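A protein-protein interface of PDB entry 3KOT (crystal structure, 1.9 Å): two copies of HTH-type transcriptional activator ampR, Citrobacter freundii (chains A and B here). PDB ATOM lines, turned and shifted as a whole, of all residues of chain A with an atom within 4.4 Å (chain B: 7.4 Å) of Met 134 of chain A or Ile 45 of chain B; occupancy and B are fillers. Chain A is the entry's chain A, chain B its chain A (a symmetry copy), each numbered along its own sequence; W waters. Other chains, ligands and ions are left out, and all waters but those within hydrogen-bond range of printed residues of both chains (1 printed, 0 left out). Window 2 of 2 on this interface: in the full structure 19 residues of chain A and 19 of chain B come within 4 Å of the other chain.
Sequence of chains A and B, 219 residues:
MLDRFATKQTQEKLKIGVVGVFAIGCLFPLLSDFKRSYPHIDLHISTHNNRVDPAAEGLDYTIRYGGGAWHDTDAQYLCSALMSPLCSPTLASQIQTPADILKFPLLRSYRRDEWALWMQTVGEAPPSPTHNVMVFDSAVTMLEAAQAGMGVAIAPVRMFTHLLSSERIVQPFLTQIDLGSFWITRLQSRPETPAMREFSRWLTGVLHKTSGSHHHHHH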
ATOM      1  N   PRO A 105     -16.557 -22.433  15.536  1.00  0.00           N
ATOM      2  CA  PRO A 105     -16.733 -23.365  14.408  1.00  0.00           C
ATOM      3  C   PRO A 105     -15.490 -23.419  13.503  1.00  0.00           C
ATOM      4  O   PRO A 105     -14.730 -22.446  13.426  1.00  0.00           O
ATOM      5  CB  PRO A 105     -17.905 -22.759  13.625  1.00  0.00           C
ATOM      6  CG  PRO A 105     -18.672 -21.963  14.630  1.00  0.00           C
ATOM      7  CD  PRO A 105     -17.624 -21.417  15.586  1.00  0.00           C
ATOM      8  N   LEU A 106     -15.284 -24.552  12.843  1.00  0.00           N
ATOM      9  CA  LEU A 106     -14.201 -24.689  11.879  1.00  0.00           C
ATOM     10  C   LEU A 106     -14.765 -24.533  10.463  1.00  0.00           C
ATOM     11  O   LEU A 106     -15.871 -24.985  10.172  1.00  0.00           O
ATOM     12  CB  LEU A 106     -13.518 -26.050  12.035  1.00  0.00           C
ATOM     13  CG  LEU A 106     -12.899 -26.358  13.412  1.00  0.00           C
ATOM     14  CD1 LEU A 106     -12.354 -27.786  13.466  1.00  0.00           C
ATOM     15  CD2 LEU A 106     -11.817 -25.350  13.780  1.00  0.00           C
ATOM     16  N   LEU A 107     -14.016 -23.862   9.599  1.00  0.00           N
ATOM     17  CA  LEU A 107     -14.378 -23.753   8.196  1.00  0.00           C
ATOM     18  C   LEU A 107     -13.367 -24.578   7.398  1.00  0.00           C
ATOM     19  O   LEU A 107     -12.158 -24.444   7.607  1.00  0.00           O
ATOM     20  CB  LEU A 107     -14.354 -22.285   7.751  1.00  0.00           C
ATOM     21  CG  LEU A 107     -14.967 -21.277   8.739  1.00  0.00           C
ATOM     22  CD1 LEU A 107     -14.783 -19.826   8.284  1.00  0.00           C
ATOM     23  CD2 LEU A 107     -16.466 -21.591   9.010  1.00  0.00           C
ATOM     24  N   ARG A 108     -13.858 -25.439   6.510  1.00  0.00           N
ATOM     25  CA  ARG A 108     -12.999 -26.336   5.726  1.00  0.00           C
ATOM     26  C   ARG A 108     -13.441 -26.399   4.261  1.00  0.00           C
ATOM     27  O   ARG A 108     -14.538 -25.960   3.907  1.00  0.00           O
ATOM     28  CB  ARG A 108     -12.985 -27.751   6.324  1.00  0.00           C
ATOM     29  CG  ARG A 108     -14.269 -28.564   6.058  1.00  0.00           C
ATOM     30  CD  ARG A 108     -14.028 -30.061   6.247  1.00  0.00           C
ATOM     31  NE  ARG A 108     -15.258 -30.856   6.262  1.00  0.00           N
ATOM     32  CZ  ARG A 108     -15.802 -31.442   5.196  1.00  0.00           C
ATOM     33  NH1 ARG A 108     -15.236 -31.318   4.003  1.00  0.00           N
ATOM     34  NH2 ARG A 108     -16.922 -32.150   5.322  1.00  0.00           N
ATOM     35  N   VAL A 133     -18.939 -27.506  12.027  1.00  0.00           N
ATOM     36  CA  VAL A 133     -18.094 -27.344  10.845  1.00  0.00           C
ATOM     37  C   VAL A 133     -18.905 -26.867   9.641  1.00  0.00           C
ATOM     38  O   VAL A 133     -19.979 -27.396   9.376  1.00  0.00           O
ATOM     39  CB  VAL A 133     -17.400 -28.676  10.491  1.00  0.00           C
ATOM     40  CG1 VAL A 133     -16.860 -28.641   9.065  1.00  0.00           C
ATOM     41  CG2 VAL A 133     -16.296 -28.986  11.494  1.00  0.00           C
ATOM     42  N   MET A 134     -18.397 -25.864   8.925  1.00  0.00           N
ATOM     43  CA  MET A 134     -18.992 -25.456   7.647  1.00  0.00           C
ATOM     44  C   MET A 134     -18.039 -25.728   6.479  1.00  0.00           C
ATOM     45  O   MET A 134     -16.825 -25.496   6.581  1.00  0.00           O
ATOM     46  CB  MET A 134     -19.408 -23.978   7.669  1.00  0.00           C
ATOM     47  CG  MET A 134     -20.542 -23.663   8.655  1.00  0.00           C
ATOM     48  SD  MET A 134     -20.888 -21.888   8.837  1.00  0.00           S
ATOM     49  CE  MET A 134     -19.804 -21.427  10.180  1.00  0.00           C
ATOM     50  N   VAL A 135     -18.605 -26.188   5.367  1.00  0.00           N
ATOM     51  CA  VAL A 135     -17.840 -26.700   4.235  1.00  0.00           C
ATOM     52  C   VAL A 135     -17.985 -25.789   3.018  1.00  0.00           C
ATOM     53  O   VAL A 135     -19.098 -25.388   2.664  1.00  0.00           O
ATOM     54  CB  VAL A 135     -18.325 -28.129   3.881  1.00  0.00           C
ATOM     55  CG1 VAL A 135     -17.533 -28.716   2.708  1.00  0.00           C
ATOM     56  CG2 VAL A 135     -18.258 -29.028   5.123  1.00  0.00           C
ATOM     57  N   PHE A 136     -16.855 -25.475   2.381  1.00  0.00           N
ATOM     58  CA  PHE A 136     -16.797 -24.502   1.296  1.00  0.00           C
ATOM     59  C   PHE A 136     -16.222 -25.058   0.008  1.00  0.00           C
ATOM     60  O   PHE A 136     -15.148 -25.669   0.016  1.00  0.00           O
ATOM     61  CB  PHE A 136     -15.953 -23.309   1.758  1.00  0.00           C
ATOM     62  CG  PHE A 136     -16.586 -22.550   2.882  1.00  0.00           C
ATOM     63  CD1 PHE A 136     -17.411 -21.473   2.619  1.00  0.00           C
ATOM     64  CD2 PHE A 136     -16.414 -22.962   4.191  1.00  0.00           C
ATOM     65  CE1 PHE A 136     -18.021 -20.798   3.637  1.00  0.00           C
ATOM     66  CE2 PHE A 136     -17.020 -22.282   5.227  1.00  0.00           C
ATOM     67  CZ  PHE A 136     -17.814 -21.194   4.960  1.00  0.00           C
ATOM     68  N   MET A 150     -17.506 -16.065  11.171  1.00  0.00           N
ATOM     69  CA  MET A 150     -18.357 -17.257  11.176  1.00  0.00           C
ATOM     70  C   MET A 150     -17.594 -18.466  11.741  1.00  0.00           C
ATOM     71  O   MET A 150     -18.186 -19.443  12.191  1.00  0.00           O
ATOM     72  CB  MET A 150     -18.887 -17.561   9.764  1.00  0.00           C
ATOM     73  CG  MET A 150     -19.918 -16.548   9.204  1.00  0.00           C
ATOM     74  SD  MET A 150     -21.382 -16.416  10.254  1.00  0.00           S
ATOM     75  CE  MET A 150     -21.971 -18.107  10.231  1.00  0.00           C
ATOM     76  N   LEU B  14     -29.609 -32.367   9.148  1.00  0.00           N
ATOM     77  CA  LEU B  14     -30.010 -31.676   7.933  1.00  0.00           C
ATOM     78  C   LEU B  14     -28.809 -31.180   7.148  1.00  0.00           C
ATOM     79  O   LEU B  14     -28.040 -30.416   7.590  1.00  0.00           O
ATOM     80  CB  LEU B  14     -30.991 -30.522   8.194  1.00  0.00           C
ATOM     81  CG  LEU B  14     -31.547 -29.648   7.113  1.00  0.00           C
ATOM     82  CD1 LEU B  14     -32.245 -30.383   6.192  1.00  0.00           C
ATOM     83  CD2 LEU B  14     -32.395 -28.637   7.666  1.00  0.00           C
ATOM     84  N   LYS B  15     -28.749 -31.620   5.923  1.00  0.00           N
ATOM     85  CA  LYS B  15     -27.667 -31.345   5.062  1.00  0.00           C
ATOM     86  C   LYS B  15     -28.149 -30.443   3.962  1.00  0.00           C
ATOM     87  O   LYS B  15     -29.041 -30.783   3.292  1.00  0.00           O
ATOM     88  CB  LYS B  15     -27.119 -32.643   4.519  1.00  0.00           C
ATOM     89  CG  LYS B  15     -25.891 -32.522   3.838  1.00  0.00           C
ATOM     90  CD  LYS B  15     -25.427 -33.817   3.206  1.00  0.00           C
ATOM     91  CE  LYS B  15     -23.966 -33.769   2.794  1.00  0.00           C
ATOM     92  NZ  LYS B  15     -23.371 -35.056   2.460  1.00  0.00           N
ATOM     93  N   ILE B  16     -27.520 -29.293   3.837  1.00  0.00           N
ATOM     94  CA  ILE B  16     -27.913 -28.237   2.922  1.00  0.00           C
ATOM     95  C   ILE B  16     -26.719 -27.657   2.124  1.00  0.00           C
ATOM     96  O   ILE B  16     -25.753 -27.265   2.667  1.00  0.00           O
ATOM     97  CB  ILE B  16     -28.682 -27.115   3.660  1.00  0.00           C
ATOM     98  CG1 ILE B  16     -29.957 -27.634   4.289  1.00  0.00           C
ATOM     99  CG2 ILE B  16     -29.039 -26.010   2.754  1.00  0.00           C
ATOM    100  CD1 ILE B  16     -30.673 -26.676   5.168  1.00  0.00           C
ATOM    101  N   GLY B  17     -26.862 -27.647   0.810  1.00  0.00           N
ATOM    102  CA  GLY B  17     -25.879 -27.053  -0.082  1.00  0.00           C
ATOM    103  C   GLY B  17     -26.346 -25.679  -0.563  1.00  0.00           C
ATOM    104  O   GLY B  17     -27.386 -25.549  -1.224  1.00  0.00           O
ATOM    105  N   VAL B  18     -25.569 -24.650  -0.240  1.00  0.00           N
ATOM    106  CA  VAL B  18     -26.018 -23.286  -0.441  1.00  0.00           C
ATOM    107  C   VAL B  18     -25.128 -22.545  -1.431  1.00  0.00           C
ATOM    108  O   VAL B  18     -23.905 -22.532  -1.296  1.00  0.00           O
ATOM    109  CB  VAL B  18     -26.071 -22.501   0.907  1.00  0.00           C
ATOM    110  CG1 VAL B  18     -26.570 -21.069   0.680  1.00  0.00           C
ATOM    111  CG2 VAL B  18     -26.960 -23.231   1.918  1.00  0.00           C
ATOM    112  N   ALA B  23     -25.144 -17.681   0.718  1.00  0.00           N
ATOM    113  CA  ALA B  23     -24.601 -17.998   2.035  1.00  0.00           C
ATOM    114  C   ALA B  23     -23.991 -16.743   2.681  1.00  0.00           C
ATOM    115  O   ALA B  23     -24.334 -16.386   3.802  1.00  0.00           O
ATOM    116  CB  ALA B  23     -23.572 -19.107   1.930  1.00  0.00           C
ATOM    117  N   LEU B  27     -27.815 -15.936   4.146  1.00  0.00           N
ATOM    118  CA  LEU B  27     -28.024 -17.015   5.126  1.00  0.00           C
ATOM    119  C   LEU B  27     -27.120 -17.016   6.349  1.00  0.00           C
ATOM    120  O   LEU B  27     -27.593 -17.224   7.468  1.00  0.00           O
ATOM    121  CB  LEU B  27     -27.961 -18.391   4.465  1.00  0.00           C
ATOM    122  CG  LEU B  27     -28.177 -19.555   5.431  1.00  0.00           C
ATOM    123  CD1 LEU B  27     -29.628 -19.526   5.963  1.00  0.00           C
ATOM    124  CD2 LEU B  27     -27.903 -20.852   4.692  1.00  0.00           C
ATOM    125  N   PHE B  28     -25.822 -16.817   6.152  1.00  0.00           N
ATOM    126  CA  PHE B  28     -24.894 -16.950   7.272  1.00  0.00           C
ATOM    127  C   PHE B  28     -25.207 -16.052   8.475  1.00  0.00           C
ATOM    128  O   PHE B  28     -25.239 -16.532   9.601  1.00  0.00           O
ATOM    129  CB  PHE B  28     -23.434 -16.831   6.818  1.00  0.00           C
ATOM    130  CG  PHE B  28     -22.913 -18.076   6.141  1.00  0.00           C
ATOM    131  CD1 PHE B  28     -23.714 -19.197   6.014  1.00  0.00           C
ATOM    132  CD2 PHE B  28     -21.619 -18.121   5.635  1.00  0.00           C
ATOM    133  CE1 PHE B  28     -23.232 -20.345   5.395  1.00  0.00           C
ATOM    134  CE2 PHE B  28     -21.143 -19.245   5.023  1.00  0.00           C
ATOM    135  CZ  PHE B  28     -21.949 -20.366   4.896  1.00  0.00           C
ATOM    136  N   LEU B  31     -28.094 -17.572  10.634  1.00  0.00           N
ATOM    137  CA  LEU B  31     -28.006 -18.943  11.131  1.00  0.00           C
ATOM    138  C   LEU B  31     -28.179 -19.074  12.649  1.00  0.00           C
ATOM    139  O   LEU B  31     -28.731 -20.061  13.109  1.00  0.00           O
ATOM    140  CB  LEU B  31     -26.698 -19.606  10.665  1.00  0.00           C
ATOM    141  CG  LEU B  31     -26.627 -20.003   9.181  1.00  0.00           C
ATOM    142  CD1 LEU B  31     -25.238 -20.509   8.816  1.00  0.00           C
ATOM    143  CD2 LEU B  31     -27.719 -21.027   8.826  1.00  0.00           C
ATOM    144  N   ASP B  42     -29.284 -30.625  13.691  1.00  0.00           N
ATOM    145  CA  ASP B  42     -27.886 -30.731  13.357  1.00  0.00           C
ATOM    146  C   ASP B  42     -27.730 -30.289  11.902  1.00  0.00           C
ATOM    147  O   ASP B  42     -27.882 -31.048  11.031  1.00  0.00           O
ATOM    148  CB  ASP B  42     -27.540 -32.202  13.424  1.00  0.00           C
ATOM    149  CG  ASP B  42     -26.168 -32.496  13.967  1.00  0.00           C
ATOM    150  OD1 ASP B  42     -25.918 -32.214  15.153  1.00  0.00           O
ATOM    151  OD2 ASP B  42     -25.394 -33.138  13.257  1.00  0.00           O
ATOM    152  N   LEU B  43     -27.391 -29.050  11.708  1.00  0.00           N
ATOM    153  CA  LEU B  43     -27.324 -28.475  10.357  1.00  0.00           C
ATOM    154  C   LEU B  43     -25.930 -28.599   9.711  1.00  0.00           C
ATOM    155  O   LEU B  43     -24.965 -28.039  10.222  1.00  0.00           O
ATOM    156  CB  LEU B  43     -27.754 -26.999  10.410  1.00  0.00           C
ATOM    157  CG  LEU B  43     -27.580 -26.132   9.166  1.00  0.00           C
ATOM    158  CD1 LEU B  43     -28.370 -26.714   8.004  1.00  0.00           C
ATOM    159  CD2 LEU B  43     -27.998 -24.689   9.439  1.00  0.00           C
ATOM    160  N   HIS B  44     -25.836 -29.321   8.608  1.00  0.00           N
ATOM    161  CA  HIS B  44     -24.591 -29.531   7.858  1.00  0.00           C
ATOM    162  C   HIS B  44     -24.534 -28.657   6.615  1.00  0.00           C
ATOM    163  O   HIS B  44     -25.008 -29.036   5.584  1.00  0.00           O
ATOM    164  CB  HIS B  44     -24.363 -31.006   7.490  1.00  0.00           C
ATOM    165  CG  HIS B  44     -24.271 -31.903   8.678  1.00  0.00           C
ATOM    166  ND1 HIS B  44     -23.279 -32.816   8.845  1.00  0.00           N
ATOM    167  CD2 HIS B  44     -25.024 -31.975   9.785  1.00  0.00           C
ATOM    168  CE1 HIS B  44     -23.436 -33.443   9.986  1.00  0.00           C
ATOM    169  NE2 HIS B  44     -24.493 -32.952  10.571  1.00  0.00           N
ATOM    170  N   ILE B  45     -23.941 -27.489   6.741  1.00  0.00           N
ATOM    171  CA  ILE B  45     -23.942 -26.526   5.642  1.00  0.00           C
ATOM    172  C   ILE B  45     -22.707 -26.665   4.782  1.00  0.00           C
ATOM    173  O   ILE B  45     -21.590 -26.784   5.293  1.00  0.00           O
ATOM    174  CB  ILE B  45     -24.031 -25.070   6.133  1.00  0.00           C
ATOM    175  CG1 ILE B  45     -25.458 -24.744   6.567  1.00  0.00           C
ATOM    176  CG2 ILE B  45     -23.635 -24.110   5.020  1.00  0.00           C
ATOM    177  CD1 ILE B  45     -25.744 -23.262   6.594  1.00  0.00           C
ATOM    178  N   SER B  46     -22.927 -26.657   3.470  1.00  0.00           N
ATOM    179  CA  SER B  46     -21.853 -26.658   2.488  1.00  0.00           C
ATOM    180  C   SER B  46     -22.198 -25.621   1.411  1.00  0.00           C
ATOM    181  O   SER B  46     -23.374 -25.306   1.200  1.00  0.00           O
ATOM    182  CB  SER B  46     -21.693 -28.044   1.871  1.00  0.00           C
ATOM    183  OG  SER B  46     -22.797 -28.364   1.042  1.00  0.00           O
ATOM    184  N   THR B  47     -21.181 -25.063   0.758  1.00  0.00           N
ATOM    185  CA  THR B  47     -21.435 -24.080  -0.291  1.00  0.00           C
ATOM    186  C   THR B  47     -21.130 -24.670  -1.673  1.00  0.00           C
ATOM    187  O   THR B  47     -20.372 -25.635  -1.803  1.00  0.00           O
ATOM    188  CB  THR B  47     -20.669 -22.738  -0.082  1.00  0.00           C
ATOM    189  OG1 THR B  47     -19.262 -22.923  -0.295  1.00  0.00           O
ATOM    190  CG2 THR B  47     -20.905 -22.148   1.318  1.00  0.00           C
ATOM    191  N   LEU B  59     -27.322 -34.231  -0.706  1.00  0.00           N
ATOM    192  CA  LEU B  59     -27.967 -33.084  -0.063  1.00  0.00           C
ATOM    193  C   LEU B  59     -29.444 -33.351   0.236  1.00  0.00           C
ATOM    194  O   LEU B  59     -30.112 -34.092  -0.494  1.00  0.00           O
ATOM    195  CB  LEU B  59     -27.821 -31.842  -0.947  1.00  0.00           C
ATOM    196  CG  LEU B  59     -26.395 -31.364  -1.265  1.00  0.00           C
ATOM    197  CD1 LEU B  59     -26.454 -30.229  -2.275  1.00  0.00           C
ATOM    198  CD2 LEU B  59     -25.674 -30.920   0.004  1.00  0.00           C
ATOM    199  N   ILE B  63     -29.990 -24.633  -1.946  1.00  0.00           N
ATOM    200  CA  ILE B  63     -30.341 -23.240  -2.172  1.00  0.00           C
ATOM    201  C   ILE B  63     -29.552 -22.740  -3.381  1.00  0.00           C
ATOM    202  O   ILE B  63     -28.333 -22.830  -3.416  1.00  0.00           O
ATOM    203  CB  ILE B  63     -30.087 -22.377  -0.918  1.00  0.00           C
ATOM    204  CG1 ILE B  63     -31.027 -22.843   0.207  1.00  0.00           C
ATOM    205  CG2 ILE B  63     -30.312 -20.910  -1.237  1.00  0.00           C
ATOM    206  CD1 ILE B  63     -30.792 -22.180   1.567  1.00  0.00           C
ATOM    207  N   PHE B 199     -36.742 -26.123   8.760  1.00  0.00           N
ATOM    208  CA  PHE B 199     -35.805 -25.192   8.149  1.00  0.00           C
ATOM    209  C   PHE B 199     -36.452 -24.339   7.047  1.00  0.00           C
ATOM    210  O   PHE B 199     -36.220 -23.132   6.980  1.00  0.00           O
ATOM    211  CB  PHE B 199     -34.572 -25.916   7.605  1.00  0.00           C
ATOM    212  CG  PHE B 199     -33.579 -24.990   6.961  1.00  0.00           C
ATOM    213  CD1 PHE B 199     -32.604 -24.360   7.723  1.00  0.00           C
ATOM    214  CD2 PHE B 199     -33.651 -24.710   5.601  1.00  0.00           C
ATOM    215  CE1 PHE B 199     -31.697 -23.480   7.127  1.00  0.00           C
ATOM    216  CE2 PHE B 199     -32.747 -23.833   5.003  1.00  0.00           C
ATOM    217  CZ  PHE B 199     -31.771 -23.222   5.773  1.00  0.00           C
HETATM  218  O   HOH W   1     -22.602 -26.772   9.184  1.00  0.00           O
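The backbone carbonyl oxygen of Val 135 of chain A lies within hydrogen-bond range of the backbone NH of Thr 47 of chain B (2.8 Å).
O of Ile 45 of chain B sits at hydrogen-bond distance from N of Val 135 of chain A, 3.0 Å away.
N of Ser 46 of chain B lies within hydrogen-bond range of O of Ile 16 of chain B.
The backbone carbonyl oxygen (O) of Ala 23 of chain B is in hydrogen-bond range of the backbone NH (N) of Phe 28 of chain B (2.8 Å).
The backbone carbonyl oxygen (O) of Met 134 of chain A sits at hydrogen-bond distance from the backbone NH (N) of Arg 108 of chain A (3.0 Å).
The backbone NH (N) of Val 18 of chain B lies within hydrogen-bond range of the backbone carbonyl oxygen (O) of Ser 46 of chain B.
The backbone carbonyl oxygen (O) of Leu 106 of chain A is in hydrogen-bond range of the backbone NH (N) of Met 134 of chain A, 3.0 Å away.
The backbone NH (N) of Phe 136 of chain A is in hydrogen-bond range of the backbone carbonyl oxygen (O) of Arg 108 of chain A, 2.8 Å away.
Of the 18 printed residues of chain B, 4 touch a printed residue of chain A.
Printed residues of chain A that touch a printed residue of chain B: Met 134, Val 135, Phe 136 and Met 150.
Hydrophobic or aromatic side chains of chain A that line the printed part of chain B: Val 135, Phe 136 and Met 150.
Among the printed residues, no Asp or Glu carboxylate lies within 4 Å of a Lys or Arg side-chain nitrogen of the other chain.
Ile 45 of chain B touches Met 134 of chain A (O to CA, 3.7 Å).
Val 135 of chain A touches Ser 46 of chain B (O to CA, 3.0 Å).
Phe 136 of chain A touches Phe 28 of chain B.
Phe 136 of chain A touches Thr 47 of chain B.
CE of Met 150 of chain A touches O of Phe 28 of chain B, 3.7 Å away.
Water W1 lies within hydrogen-bond range of O of Val 133 of chain A, O of Leu 43 of chain B and N of Ile 45 of chain B.
No position is printed for both chains.
Of the 7 pairs that touch across the chains among the printed residues, none has its exchanged pair printed and touching as well.
Of chain B, only Ile 45 (3.7 Å) comes within 4 Å of Met 134 of chain A.
Printed residues of chain B within 4 Å of Val 135 of chain A: Ile 45, Ser 46 and Thr 47.
Printed residues of chain A within 4 Å of Phe 28 of chain B: Phe 136 (3.8 Å) and Met 150 (3.7 Å).
Ile 45 of chain B touches just these residues of chain A: Met 134 and Val 135.
Phe 199 of chain B touches none of the printed residues of chain A.
The nearest printed residue of chain A that does not touch Thr 47 of chain B is Met 134 of chain A (6.6 Å).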
